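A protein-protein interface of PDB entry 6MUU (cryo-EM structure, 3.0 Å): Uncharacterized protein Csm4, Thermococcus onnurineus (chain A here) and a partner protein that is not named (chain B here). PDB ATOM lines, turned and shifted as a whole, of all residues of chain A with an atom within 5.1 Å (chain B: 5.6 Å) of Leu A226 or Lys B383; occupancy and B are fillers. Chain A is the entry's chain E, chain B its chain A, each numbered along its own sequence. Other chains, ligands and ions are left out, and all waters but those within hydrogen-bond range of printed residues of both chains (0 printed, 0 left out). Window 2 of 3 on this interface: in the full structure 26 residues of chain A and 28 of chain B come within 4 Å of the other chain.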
ATOM      1  N   LEU A  71      14.975  22.975 -21.470  1.00  0.00           N
ATOM      2  CA  LEU A  71      15.461  22.982 -22.838  1.00  0.00           C
ATOM      3  C   LEU A  71      16.908  22.538 -22.950  1.00  0.00           C
ATOM      4  O   LEU A  71      17.483  22.609 -24.039  1.00  0.00           O
ATOM      5  CB  LEU A  71      15.277  24.358 -23.476  1.00  0.00           C
ATOM      6  CG  LEU A  71      13.970  24.561 -24.241  1.00  0.00           C
ATOM      7  CD1 LEU A  71      12.739  24.644 -23.360  1.00  0.00           C
ATOM      8  CD2 LEU A  71      14.098  25.799 -25.052  1.00  0.00           C
ATOM      9  N   SER A  72      17.502  22.061 -21.858  1.00  0.00           N
ATOM     10  CA  SER A  72      18.871  21.573 -21.873  1.00  0.00           C
ATOM     11  C   SER A  72      18.976  20.142 -22.361  1.00  0.00           C
ATOM     12  O   SER A  72      20.077  19.690 -22.686  1.00  0.00           O
ATOM     13  CB  SER A  72      19.470  21.662 -20.473  1.00  0.00           C
ATOM     14  OG  SER A  72      20.816  21.241 -20.472  1.00  0.00           O
ATOM     15  N   PRO A  75      19.889  19.274 -26.814  1.00  0.00           N
ATOM     16  CA  PRO A  75      21.186  19.100 -27.490  1.00  0.00           C
ATOM     17  C   PRO A  75      21.879  17.776 -27.210  1.00  0.00           C
ATOM     18  O   PRO A  75      22.374  17.132 -28.139  1.00  0.00           O
ATOM     19  CB  PRO A  75      22.017  20.274 -26.962  1.00  0.00           C
ATOM     20  CG  PRO A  75      21.049  21.286 -26.625  1.00  0.00           C
ATOM     21  CD  PRO A  75      19.895  20.546 -26.061  1.00  0.00           C
ATOM     22  N   PRO A 224      19.829  35.124 -24.100  1.00  0.00           N
ATOM     23  CA  PRO A 224      19.829  33.882 -23.323  1.00  0.00           C
ATOM     24  C   PRO A 224      20.728  32.819 -23.928  1.00  0.00           C
ATOM     25  O   PRO A 224      21.469  33.085 -24.876  1.00  0.00           O
ATOM     26  CB  PRO A 224      18.359  33.450 -23.363  1.00  0.00           C
ATOM     27  CG  PRO A 224      17.612  34.671 -23.747  1.00  0.00           C
ATOM     28  CD  PRO A 224      18.502  35.412 -24.656  1.00  0.00           C
ATOM     29  N   VAL A 225      20.728  31.618 -23.350  1.00  0.00           N
ATOM     30  CA  VAL A 225      21.610  30.527 -23.871  1.00  0.00           C
ATOM     31  C   VAL A 225      20.802  29.587 -24.773  1.00  0.00           C
ATOM     32  O   VAL A 225      21.214  29.379 -25.919  1.00  0.00           O
ATOM     33  CB  VAL A 225      22.246  29.740 -22.711  1.00  0.00           C
ATOM     34  CG1 VAL A 225      23.185  28.662 -23.219  1.00  0.00           C
ATOM     35  CG2 VAL A 225      22.967  30.651 -21.732  1.00  0.00           C
ATOM     36  N   LEU A 226      19.731  29.004 -24.260  1.00  0.00           N
ATOM     37  CA  LEU A 226      18.809  28.140 -25.044  1.00  0.00           C
ATOM     38  C   LEU A 226      17.405  28.672 -24.763  1.00  0.00           C
ATOM     39  O   LEU A 226      17.125  28.900 -23.582  1.00  0.00           O
ATOM     40  CB  LEU A 226      18.942  26.691 -24.575  1.00  0.00           C
ATOM     41  CG  LEU A 226      20.205  25.963 -25.024  1.00  0.00           C
ATOM     42  CD1 LEU A 226      20.387  24.677 -24.239  1.00  0.00           C
ATOM     43  CD2 LEU A 226      20.167  25.676 -26.515  1.00  0.00           C
ATOM     44  N   TRP A 227      16.538  28.850 -25.744  1.00  0.00           N
ATOM     45  CA  TRP A 227      15.227  29.446 -25.388  1.00  0.00           C
ATOM     46  C   TRP A 227      14.143  29.079 -26.396  1.00  0.00           C
ATOM     47  O   TRP A 227      14.445  28.443 -27.411  1.00  0.00           O
ATOM     48  CB  TRP A 227      15.367  30.965 -25.289  1.00  0.00           C
ATOM     49  CG  TRP A 227      15.604  31.632 -26.607  1.00  0.00           C
ATOM     50  CD1 TRP A 227      14.662  32.010 -27.516  1.00  0.00           C
ATOM     51  CD2 TRP A 227      16.872  32.020 -27.162  1.00  0.00           C
ATOM     52  NE1 TRP A 227      15.254  32.600 -28.598  1.00  0.00           N
ATOM     53  CE2 TRP A 227      16.609  32.622 -28.409  1.00  0.00           C
ATOM     54  CE3 TRP A 227      18.196  31.917 -26.733  1.00  0.00           C
ATOM     55  CZ2 TRP A 227      17.623  33.120 -29.222  1.00  0.00           C
ATOM     56  CZ3 TRP A 227      19.198  32.405 -27.539  1.00  0.00           C
ATOM     57  CH2 TRP A 227      18.912  32.999 -28.766  1.00  0.00           C
ATOM     58  N   ARG A 228      12.920  29.406 -26.031  1.00  0.00           N
ATOM     59  CA  ARG A 228      11.760  29.255 -26.892  1.00  0.00           C
ATOM     60  C   ARG A 228      10.961  30.541 -26.807  1.00  0.00           C
ATOM     61  O   ARG A 228      10.609  30.978 -25.711  1.00  0.00           O
ATOM     62  CB  ARG A 228      10.897  28.063 -26.480  1.00  0.00           C
ATOM     63  CG  ARG A 228       9.749  27.805 -27.429  1.00  0.00           C
ATOM     64  CD  ARG A 228       8.983  26.533 -27.106  1.00  0.00           C
ATOM     65  NE  ARG A 228       8.204  26.618 -25.875  1.00  0.00           N
ATOM     66  CZ  ARG A 228       8.437  25.895 -24.786  1.00  0.00           C
ATOM     67  NH1 ARG A 228       9.438  25.027 -24.763  1.00  0.00           N
ATOM     68  NH2 ARG A 228       7.669  26.039 -23.717  1.00  0.00           N
ATOM     69  N   SER A 251      13.352  27.787 -20.390  1.00  0.00           N
ATOM     70  CA  SER A 251      14.453  28.368 -21.126  1.00  0.00           C
ATOM     71  C   SER A 251      15.583  28.724 -20.177  1.00  0.00           C
ATOM     72  O   SER A 251      15.381  28.932 -18.981  1.00  0.00           O
ATOM     73  CB  SER A 251      13.981  29.590 -21.884  1.00  0.00           C
ATOM     74  OG  SER A 251      12.983  29.216 -22.807  1.00  0.00           O
ATOM     75  N   ILE A 252      16.787  28.792 -20.727  1.00  0.00           N
ATOM     76  CA  ILE A 252      18.013  28.721 -19.951  1.00  0.00           C
ATOM     77  C   ILE A 252      18.740  30.048 -20.051  1.00  0.00           C
ATOM     78  O   ILE A 252      19.070  30.505 -21.151  1.00  0.00           O
ATOM     79  CB  ILE A 252      18.890  27.569 -20.437  1.00  0.00           C
ATOM     80  CG1 ILE A 252      18.131  26.265 -20.259  1.00  0.00           C
ATOM     81  CG2 ILE A 252      20.187  27.545 -19.689  1.00  0.00           C
ATOM     82  CD1 ILE A 252      18.704  25.179 -21.024  1.00  0.00           C
ATOM     83  N   LEU A 284      24.350  22.283 -18.270  1.00  0.00           N
ATOM     84  CA  LEU A 284      24.290  22.265 -19.718  1.00  0.00           C
ATOM     85  C   LEU A 284      25.170  21.159 -20.282  1.00  0.00           C
ATOM     86  O   LEU A 284      26.088  20.680 -19.616  1.00  0.00           O
ATOM     87  CB  LEU A 284      24.730  23.608 -20.299  1.00  0.00           C
ATOM     88  CG  LEU A 284      23.837  24.838 -20.220  1.00  0.00           C
ATOM     89  CD1 LEU A 284      24.521  25.936 -20.985  1.00  0.00           C
ATOM     90  CD2 LEU A 284      22.476  24.576 -20.801  1.00  0.00           C
ATOM     91  N   TYR B 344      10.727  30.618 -39.199  1.00  0.00           N
ATOM     92  CA  TYR B 344      12.159  30.829 -39.072  1.00  0.00           C
ATOM     93  C   TYR B 344      12.924  29.773 -39.845  1.00  0.00           C
ATOM     94  O   TYR B 344      12.549  28.600 -39.848  1.00  0.00           O
ATOM     95  CB  TYR B 344      12.582  30.826 -37.604  1.00  0.00           C
ATOM     96  CG  TYR B 344      14.071  30.815 -37.383  1.00  0.00           C
ATOM     97  CD1 TYR B 344      14.872  31.860 -37.821  1.00  0.00           C
ATOM     98  CD2 TYR B 344      14.666  29.787 -36.675  1.00  0.00           C
ATOM     99  CE1 TYR B 344      16.231  31.842 -37.616  1.00  0.00           C
ATOM    100  CE2 TYR B 344      16.016  29.768 -36.454  1.00  0.00           C
ATOM    101  CZ  TYR B 344      16.789  30.803 -36.916  1.00  0.00           C
ATOM    102  OH  TYR B 344      18.135  30.786 -36.692  1.00  0.00           O
ATOM    103  N   VAL B 379      20.549  22.793 -32.359  1.00  0.00           N
ATOM    104  CA  VAL B 379      20.987  23.893 -31.507  1.00  0.00           C
ATOM    105  C   VAL B 379      20.522  25.226 -32.073  1.00  0.00           C
ATOM    106  O   VAL B 379      20.147  26.133 -31.323  1.00  0.00           O
ATOM    107  CB  VAL B 379      22.517  23.832 -31.344  1.00  0.00           C
ATOM    108  CG1 VAL B 379      23.041  24.988 -30.519  1.00  0.00           C
ATOM    109  CG2 VAL B 379      22.924  22.521 -30.710  1.00  0.00           C
ATOM    110  N   ARG B 380      20.485  25.351 -33.397  1.00  0.00           N
ATOM    111  CA  ARG B 380      20.054  26.600 -34.006  1.00  0.00           C
ATOM    112  C   ARG B 380      18.546  26.803 -33.874  1.00  0.00           C
ATOM    113  O   ARG B 380      18.085  27.941 -33.753  1.00  0.00           O
ATOM    114  CB  ARG B 380      20.511  26.633 -35.466  1.00  0.00           C
ATOM    115  CG  ARG B 380      20.139  27.882 -36.217  1.00  0.00           C
ATOM    116  CD  ARG B 380      20.692  29.109 -35.544  1.00  0.00           C
ATOM    117  NE  ARG B 380      22.142  29.191 -35.602  1.00  0.00           N
ATOM    118  CZ  ARG B 380      22.803  29.759 -36.599  1.00  0.00           C
ATOM    119  NH1 ARG B 380      22.137  30.282 -37.611  1.00  0.00           N
ATOM    120  NH2 ARG B 380      24.125  29.795 -36.587  1.00  0.00           N
ATOM    121  N   LYS B 381      17.767  25.725 -33.847  1.00  0.00           N
ATOM    122  CA  LYS B 381      16.333  25.855 -33.620  1.00  0.00           C
ATOM    123  C   LYS B 381      15.998  26.228 -32.185  1.00  0.00           C
ATOM    124  O   LYS B 381      14.884  26.695 -31.931  1.00  0.00           O
ATOM    125  CB  LYS B 381      15.614  24.561 -33.970  1.00  0.00           C
ATOM    126  CG  LYS B 381      15.560  24.252 -35.436  1.00  0.00           C
ATOM    127  CD  LYS B 381      14.916  22.906 -35.645  1.00  0.00           C
ATOM    128  CE  LYS B 381      15.001  22.471 -37.078  1.00  0.00           C
ATOM    129  NZ  LYS B 381      14.140  23.316 -37.929  1.00  0.00           N
ATOM    130  N   LEU B 382      16.913  26.026 -31.244  1.00  0.00           N
ATOM    131  CA  LEU B 382      16.717  26.458 -29.868  1.00  0.00           C
ATOM    132  C   LEU B 382      17.201  27.876 -29.624  1.00  0.00           C
ATOM    133  O   LEU B 382      17.187  28.335 -28.482  1.00  0.00           O
ATOM    134  CB  LEU B 382      17.419  25.504 -28.910  1.00  0.00           C
ATOM    135  CG  LEU B 382      16.804  24.115 -28.828  1.00  0.00           C
ATOM    136  CD1 LEU B 382      17.678  23.224 -27.986  1.00  0.00           C
ATOM    137  CD2 LEU B 382      15.418  24.183 -28.250  1.00  0.00           C
ATOM    138  N   LYS B 383      17.642  28.566 -30.665  1.00  0.00           N
ATOM    139  CA  LYS B 383      18.016  29.974 -30.629  1.00  0.00           C
ATOM    140  C   LYS B 383      17.302  30.611 -31.810  1.00  0.00           C
ATOM    141  O   LYS B 383      17.912  30.783 -32.863  1.00  0.00           O
ATOM    142  CB  LYS B 383      19.512  30.130 -30.749  1.00  0.00           C
ATOM    143  CG  LYS B 383      20.332  29.540 -29.636  1.00  0.00           C
ATOM    144  CD  LYS B 383      21.796  29.696 -29.980  1.00  0.00           C
ATOM    145  CE  LYS B 383      22.678  29.259 -28.848  1.00  0.00           C
ATOM    146  NZ  LYS B 383      22.546  27.808 -28.583  1.00  0.00           N
ATOM    147  N   ARG B 384      16.031  30.981 -31.638  1.00  0.00           N
ATOM    148  CA  ARG B 384      15.201  31.143 -32.825  1.00  0.00           C
ATOM    149  C   ARG B 384      15.429  32.448 -33.562  1.00  0.00           C
ATOM    150  O   ARG B 384      15.275  32.471 -34.775  1.00  0.00           O
ATOM    151  CB  ARG B 384      13.716  31.009 -32.507  1.00  0.00           C
ATOM    152  CG  ARG B 384      13.321  29.621 -32.093  1.00  0.00           C
ATOM    153  CD  ARG B 384      11.813  29.413 -32.125  1.00  0.00           C
ATOM    154  NE  ARG B 384      11.314  29.210 -33.485  1.00  0.00           N
ATOM    155  CZ  ARG B 384      10.549  30.070 -34.143  1.00  0.00           C
ATOM    156  NH1 ARG B 384      10.194  31.208 -33.573  1.00  0.00           N
ATOM    157  NH2 ARG B 384      10.141  29.790 -35.371  1.00  0.00           N
ATOM    158  N   PHE B 385      15.741  33.545 -32.901  1.00  0.00           N
ATOM    159  CA  PHE B 385      16.071  34.752 -33.652  1.00  0.00           C
ATOM    160  C   PHE B 385      17.248  35.461 -33.006  1.00  0.00           C
ATOM    161  O   PHE B 385      17.201  36.657 -32.725  1.00  0.00           O
ATOM    162  CB  PHE B 385      14.858  35.662 -33.810  1.00  0.00           C
ATOM    163  CG  PHE B 385      13.893  35.207 -34.866  1.00  0.00           C
ATOM    164  CD1 PHE B 385      14.116  35.515 -36.193  1.00  0.00           C
ATOM    165  CD2 PHE B 385      12.782  34.455 -34.545  1.00  0.00           C
ATOM    166  CE1 PHE B 385      13.245  35.098 -37.171  1.00  0.00           C
ATOM    167  CE2 PHE B 385      11.918  34.024 -35.529  1.00  0.00           C
ATOM    168  CZ  PHE B 385      12.145  34.357 -36.836  1.00  0.00           C
ATOM    169  N   GLY B 386      18.312  34.706 -32.727  1.00  0.00           N
ATOM    170  CA  GLY B 386      19.470  35.269 -32.061  1.00  0.00           C
ATOM    171  C   GLY B 386      20.229  36.281 -32.887  1.00  0.00           C
ATOM    172  O   GLY B 386      20.919  37.136 -32.323  1.00  0.00           O
ATOM    173  N   GLU B 387      20.113  36.210 -34.205  1.00  0.00           N
ATOM    174  CA  GLU B 387      20.784  37.134 -35.116  1.00  0.00           C
ATOM    175  C   GLU B 387      19.891  38.311 -35.510  1.00  0.00           C
ATOM    176  O   GLU B 387      19.738  38.645 -36.682  1.00  0.00           O
ATOM    177  CB  GLU B 387      21.292  36.366 -36.336  1.00  0.00           C
ATOM    178  CG  GLU B 387      20.257  35.523 -37.099  1.00  0.00           C
ATOM    179  CD  GLU B 387      20.150  34.098 -36.585  1.00  0.00           C
ATOM    180  OE1 GLU B 387      20.632  33.828 -35.469  1.00  0.00           O
ATOM    181  OE2 GLU B 387      19.585  33.246 -37.296  1.00  0.00           O
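O of Leu B382 lies within hydrogen-bond range of N of Trp A227, 2.9 Å away.
The side-chain amino group (NZ) of Lys B383 lies close to the backbone carbonyl oxygen (O) of Val A225 (3.4 Å).
The backbone NH (N) of Val A225 sits at hydrogen-bond distance from the backbone carbonyl oxygen (O) of Ile A252 (3.0 Å).
The backbone carbonyl oxygen (O) of Leu A226 sits at hydrogen-bond distance from the backbone NH (N) of Ile A252 (2.9 Å).
Among the printed residues, pairs that only touch across the chains: Leu A71 with Leu B382 (3.8 Å), Pro A75 with Leu B382 (3.97 Å), Leu A226 with Leu B382 (3.6 Å), Leu A226 with Lys B383 (3.8 Å), Trp A227 with Lys B383 (3.5 Å), Trp A227 with Arg B384 (3.5 Å) and Trp A227 with Gly B386 (3.9 Å).
Printed residues of chain B within 4 Å of Pro A75: Leu B382 (3.97 Å).
Leu A226 touches just these residues of chain B: Leu B382 and Lys B383.
Val B379 touches none of the printed residues of chain A.
Of chain A, only Val A225 (3.3 Å), Leu A226 (3.8 Å) and Trp A227 (3.5 Å) come within 4 Å of Lys B383.
Of the printed residues of chain A, Arg B384 touches Trp A227 (3.5 Å).
Of the printed residues of chain A, Gly B386 touches Trp A227.
The nearest residue of chain B that does not touch Leu A226 is Val B379 (4.8 Å).
The nearest printed residue of chain A that does not touch Lys B383 is Pro A224 (5.6 Å).
Of the 10 printed residues of chain B, 4 touch a printed residue of chain A.
Hydrophobic or aromatic side chains of chain B that line the printed part of chain A: Leu B382.
Printed residues of chain A that touch a printed residue of chain B: Leu A71, Pro A75, Val A225, Leu A226 and Trp A227.
Among the printed residues, 9 pairs touch across the chains.
Among the printed residues, no Asp or Glu carboxylate lies within 4 Å of a Lys or Arg side-chain nitrogen of the other chain.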
